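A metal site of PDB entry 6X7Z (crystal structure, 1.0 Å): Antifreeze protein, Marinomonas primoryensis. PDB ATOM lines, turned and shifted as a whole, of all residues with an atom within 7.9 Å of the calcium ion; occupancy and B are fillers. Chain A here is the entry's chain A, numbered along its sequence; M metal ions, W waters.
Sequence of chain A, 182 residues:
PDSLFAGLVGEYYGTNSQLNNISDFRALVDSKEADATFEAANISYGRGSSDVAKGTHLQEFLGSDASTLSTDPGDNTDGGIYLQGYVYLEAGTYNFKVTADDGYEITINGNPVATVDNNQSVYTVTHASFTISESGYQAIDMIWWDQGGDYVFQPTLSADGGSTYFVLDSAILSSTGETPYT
The side-chain carboxylate (OD2) of Asp 78 sits close to the backbone NH (N) of Leu 19 (3.0 Å).
The side-chain amide nitrogen of Asn 119 sits close to the side-chain amide oxygen of Gln 147.
The side-chain amide nitrogen (NE2) of Gln 18 lies within hydrogen-bond range of the side-chain amide oxygen (OD1) of Asn 20, at 2.9 Å.
O of Asp 78 lies within hydrogen-bond range of N of Thr 15 (2.9 Å).
The side-chain amide nitrogen of Gln 18 sits close to the side-chain amide nitrogen of Asn 119 (3.4 Å).
The backbone NH (N) of Gln 147 sits close to the side-chain carboxylate (OD2) of Asp 102.
OG1 of Thr 77 sits close to OD1 of Asp 78, 2.7 Å away.
Three residues have an atom within 4 Å of the calcium ion: Gln 18, Asp 78 and Gln 147.
The nearest printed residue that does not touch the calcium ion is Thr 77 (4.5 Å).
The calcium ion is bound by the side-chain amide oxygen (OE1) of Gln 18, the backbone carbonyl oxygen (O) of Gln 147, water W1, water W3, the side-chain carboxylate (OD1) of Asp 78, water W2 and the side-chain carboxylate (OD2) of Asp 78.
The calcium ion has seven donor atoms within binding distance.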
ATOM      1  N   THR A  15      19.280   5.207  23.820  1.00  0.00           N
ATOM      2  CA  THR A  15      17.829   5.049  23.761  1.00  0.00           C
ATOM      3  C   THR A  15      17.357   4.355  25.032  1.00  0.00           C
ATOM      4  O   THR A  15      18.107   3.645  25.686  1.00  0.00           O
ATOM      5  CB  THR A  15      17.432   4.242  22.498  1.00  0.00           C
ATOM      6  OG1 THR A  15      15.999   4.146  22.406  1.00  0.00           O
ATOM      7  CG2 THR A  15      17.948   2.823  22.486  1.00  0.00           C
ATOM      8  N   ASN A  16      16.055   4.534  25.343  1.00  0.00           N
ATOM      9  CA  ASN A  16      15.422   3.797  26.424  1.00  0.00           C
ATOM     10  C   ASN A  16      14.508   2.690  25.897  1.00  0.00           C
ATOM     11  O   ASN A  16      13.759   2.074  26.672  1.00  0.00           O
ATOM     12  CB  ASN A  16      14.698   4.736  27.381  1.00  0.00           C
ATOM     13  CG  ASN A  16      15.644   5.766  27.947  1.00  0.00           C
ATOM     14  OD1 ASN A  16      16.790   5.415  28.372  1.00  0.00           O
ATOM     15  ND2 ASN A  16      15.251   6.986  28.003  1.00  0.00           N
ATOM     16  N   SER A  17      14.583   2.419  24.598  1.00  0.00           N
ATOM     17  CA  SER A  17      13.995   1.254  23.976  1.00  0.00           C
ATOM     18  C   SER A  17      15.036   0.120  23.914  1.00  0.00           C
ATOM     19  O   SER A  17      16.235   0.351  24.049  1.00  0.00           O
ATOM     20  CB  SER A  17      13.512   1.596  22.586  1.00  0.00           C
ATOM     21  OG  SER A  17      14.574   1.837  21.668  1.00  0.00           O
ATOM     22  N   GLN A  18      14.534  -1.099  23.694  1.00  0.00           N
ATOM     23  CA  GLN A  18      15.427  -2.247  23.618  1.00  0.00           C
ATOM     24  C   GLN A  18      16.068  -2.358  22.229  1.00  0.00           C
ATOM     25  O   GLN A  18      15.382  -2.337  21.185  1.00  0.00           O
ATOM     26  CB  GLN A  18      14.630  -3.531  23.904  1.00  0.00           C
ATOM     27  CG  GLN A  18      15.367  -4.843  23.606  1.00  0.00           C
ATOM     28  CD  GLN A  18      16.563  -5.152  24.468  1.00  0.00           C
ATOM     29  OE1 GLN A  18      17.031  -4.306  25.252  1.00  0.00           O
ATOM     30  NE2 GLN A  18      17.074  -6.354  24.361  1.00  0.00           N
ATOM     31  N   LEU A  19      17.373  -2.577  22.212  1.00  0.00           N
ATOM     32  CA  LEU A  19      18.119  -2.925  21.011  1.00  0.00           C
ATOM     33  C   LEU A  19      18.322  -4.430  20.978  1.00  0.00           C
ATOM     34  O   LEU A  19      19.058  -4.981  21.799  1.00  0.00           O
ATOM     35  CB  LEU A  19      19.446  -2.181  20.984  1.00  0.00           C
ATOM     36  CG  LEU A  19      19.361  -0.660  20.979  1.00  0.00           C
ATOM     37  CD1 LEU A  19      20.764  -0.057  21.090  1.00  0.00           C
ATOM     38  CD2 LEU A  19      18.654  -0.154  19.730  1.00  0.00           C
ATOM     39  N   ASN A  20      17.649  -5.112  20.014  1.00  0.00           N
ATOM     40  CA  ASN A  20      17.767  -6.560  19.895  1.00  0.00           C
ATOM     41  C   ASN A  20      18.660  -7.016  18.738  1.00  0.00           C
ATOM     42  O   ASN A  20      19.055  -8.175  18.706  1.00  0.00           O
ATOM     43  CB  ASN A  20      16.397  -7.213  19.691  1.00  0.00           C
ATOM     44  CG  ASN A  20      15.596  -7.285  20.984  1.00  0.00           C
ATOM     45  OD1 ASN A  20      16.134  -7.762  22.005  1.00  0.00           O
ATOM     46  ND2 ASN A  20      14.362  -6.894  20.929  1.00  0.00           N
ATOM     47  N   ASP A  51      25.995  -1.157  32.002  1.00  0.00           N
ATOM     48  CA  ASP A  51      25.302  -0.470  30.867  1.00  0.00           C
ATOM     49  C   ASP A  51      26.185   0.610  30.245  1.00  0.00           C
ATOM     50  O   ASP A  51      26.547   1.589  30.897  1.00  0.00           O
ATOM     51  CB  ASP A  51      23.978   0.160  31.275  1.00  0.00           C
ATOM     52  CG  ASP A  51      23.016  -0.729  32.018  1.00  0.00           C
ATOM     53  OD1 ASP A  51      22.915  -1.907  31.706  1.00  0.00           O
ATOM     54  OD2 ASP A  51      22.226  -0.149  32.767  1.00  0.00           O
ATOM     55  N   THR A  77      19.142   3.533  28.749  1.00  0.00           N
ATOM     56  CA  THR A  77      19.297   2.101  29.091  1.00  0.00           C
ATOM     57  C   THR A  77      20.184   1.366  28.092  1.00  0.00           C
ATOM     58  O   THR A  77      20.900   0.431  28.474  1.00  0.00           O
ATOM     59  CB  THR A  77      17.921   1.416  29.211  1.00  0.00           C
ATOM     60  OG1 THR A  77      17.253   1.370  27.965  1.00  0.00           O
ATOM     61  CG2 THR A  77      17.025   2.122  30.214  1.00  0.00           C
ATOM     62  N   ASP A  78      20.093   1.749  26.810  1.00  0.00           N
ATOM     63  CA  ASP A  78      20.703   1.060  25.703  1.00  0.00           C
ATOM     64  C   ASP A  78      21.473   2.070  24.853  1.00  0.00           C
ATOM     65  O   ASP A  78      21.100   3.260  24.847  1.00  0.00           O
ATOM     66  CB  ASP A  78      19.636   0.375  24.807  1.00  0.00           C
ATOM     67  CG  ASP A  78      18.883  -0.771  25.451  1.00  0.00           C
ATOM     68  OD1 ASP A  78      18.387  -0.615  26.615  1.00  0.00           O
ATOM     69  OD2 ASP A  78      18.756  -1.854  24.824  1.00  0.00           O
ATOM     70  N   GLY A  79      22.518   1.646  24.155  1.00  0.00           N
ATOM     71  CA  GLY A  79      23.189   2.609  23.295  1.00  0.00           C
ATOM     72  C   GLY A  79      24.194   1.931  22.407  1.00  0.00           C
ATOM     73  O   GLY A  79      24.500   0.755  22.578  1.00  0.00           O
ATOM     74  N   ASP A 102      27.303  -6.088  22.772  1.00  0.00           N
ATOM     75  CA  ASP A 102      26.406  -7.074  22.170  1.00  0.00           C
ATOM     76  C   ASP A 102      26.838  -7.341  20.723  1.00  0.00           C
ATOM     77  O   ASP A 102      27.925  -7.860  20.512  1.00  0.00           O
ATOM     78  CB  ASP A 102      24.951  -6.621  22.376  1.00  0.00           C
ATOM     79  CG  ASP A 102      24.525  -6.880  23.808  1.00  0.00           C
ATOM     80  OD1 ASP A 102      24.200  -8.062  24.106  1.00  0.00           O
ATOM     81  OD2 ASP A 102      24.536  -5.923  24.648  1.00  0.00           O
ATOM     82  N   ASN A 119      21.949  -9.980  20.345  1.00  0.00           N
ATOM     83  CA  ASN A 119      22.604  -9.722  21.610  1.00  0.00           C
ATOM     84  C   ASN A 119      23.413 -10.932  22.024  1.00  0.00           C
ATOM     85  O   ASN A 119      23.142 -12.059  21.609  1.00  0.00           O
ATOM     86  CB  ASN A 119      21.569  -9.343  22.659  1.00  0.00           C
ATOM     87  CG  ASN A 119      21.006  -7.952  22.379  1.00  0.00           C
ATOM     88  OD1 ASN A 119      21.731  -7.090  21.913  1.00  0.00           O
ATOM     89  ND2 ASN A 119      19.739  -7.732  22.690  1.00  0.00           N
ATOM     90  N   TRP A 145      26.423  -2.193  19.375  1.00  0.00           N
ATOM     91  CA  TRP A 145      25.568  -1.682  20.449  1.00  0.00           C
ATOM     92  C   TRP A 145      25.659  -2.550  21.685  1.00  0.00           C
ATOM     93  O   TRP A 145      26.132  -3.685  21.644  1.00  0.00           O
ATOM     94  CB  TRP A 145      24.089  -1.557  19.975  1.00  0.00           C
ATOM     95  CG  TRP A 145      23.392  -2.880  19.870  1.00  0.00           C
ATOM     96  CD1 TRP A 145      22.688  -3.497  20.868  1.00  0.00           C
ATOM     97  CD2 TRP A 145      23.443  -3.828  18.796  1.00  0.00           C
ATOM     98  NE1 TRP A 145      22.272  -4.748  20.488  1.00  0.00           N
ATOM     99  CE2 TRP A 145      22.732  -4.970  19.213  1.00  0.00           C
ATOM    100  CE3 TRP A 145      23.988  -3.803  17.518  1.00  0.00           C
ATOM    101  CZ2 TRP A 145      22.610  -6.120  18.404  1.00  0.00           C
ATOM    102  CZ3 TRP A 145      23.864  -4.931  16.720  1.00  0.00           C
ATOM    103  CH2 TRP A 145      23.192  -6.065  17.160  1.00  0.00           C
ATOM    104  N   ASP A 146      25.114  -1.966  22.749  1.00  0.00           N
ATOM    105  CA  ASP A 146      24.904  -2.607  24.041  1.00  0.00           C
ATOM    106  C   ASP A 146      23.411  -2.502  24.386  1.00  0.00           C
ATOM    107  O   ASP A 146      22.850  -1.423  24.466  1.00  0.00           O
ATOM    108  CB  ASP A 146      25.703  -1.914  25.139  1.00  0.00           C
ATOM    109  CG  ASP A 146      25.442  -2.467  26.529  1.00  0.00           C
ATOM    110  OD1 ASP A 146      25.253  -3.725  26.590  1.00  0.00           O
ATOM    111  OD2 ASP A 146      25.379  -1.708  27.496  1.00  0.00           O
ATOM    112  N   GLN A 147      22.781  -3.677  24.592  1.00  0.00           N
ATOM    113  CA  GLN A 147      21.382  -3.729  25.080  1.00  0.00           C
ATOM    114  C   GLN A 147      21.299  -3.507  26.586  1.00  0.00           C
ATOM    115  O   GLN A 147      20.196  -3.398  27.127  1.00  0.00           O
ATOM    116  CB  GLN A 147      20.708  -5.084  24.778  1.00  0.00           C
ATOM    117  CG  GLN A 147      21.229  -6.241  25.622  1.00  0.00           C
ATOM    118  CD  GLN A 147      20.269  -7.386  25.875  1.00  0.00           C
ATOM    119  OE1 GLN A 147      19.074  -7.129  26.065  1.00  0.00           O
ATOM    120  NE2 GLN A 147      20.749  -8.602  25.929  1.00  0.00           N
ATOM    121  N   GLY A 148      22.440  -3.500  27.266  1.00  0.00           N
ATOM    122  CA  GLY A 148      22.504  -3.435  28.708  1.00  0.00           C
ATOM    123  C   GLY A 148      23.508  -4.425  29.246  1.00  0.00           C
ATOM    124  O   GLY A 148      23.873  -5.414  28.581  1.00  0.00           O
ATOM    125  N   GLY A 149      23.935  -4.195  30.487  1.00  0.00           N
ATOM    126  CA  GLY A 149      24.836  -5.090  31.173  1.00  0.00           C
ATOM    127  C   GLY A 149      26.291  -4.811  30.835  1.00  0.00           C
ATOM    128  O   GLY A 149      26.768  -3.687  30.968  1.00  0.00           O
HETATM  129 CA    CA M   1      17.913  -2.962  26.903  1.00  0.00          CA
HETATM  130  O   HOH W   1      15.626  -2.410  27.083  1.00  0.00           O
HETATM  131  O   HOH W   2      17.802  -5.138  28.013  1.00  0.00           O
HETATM  132  O   HOH W   3      17.920  -2.467  29.254  1.00  0.00           O
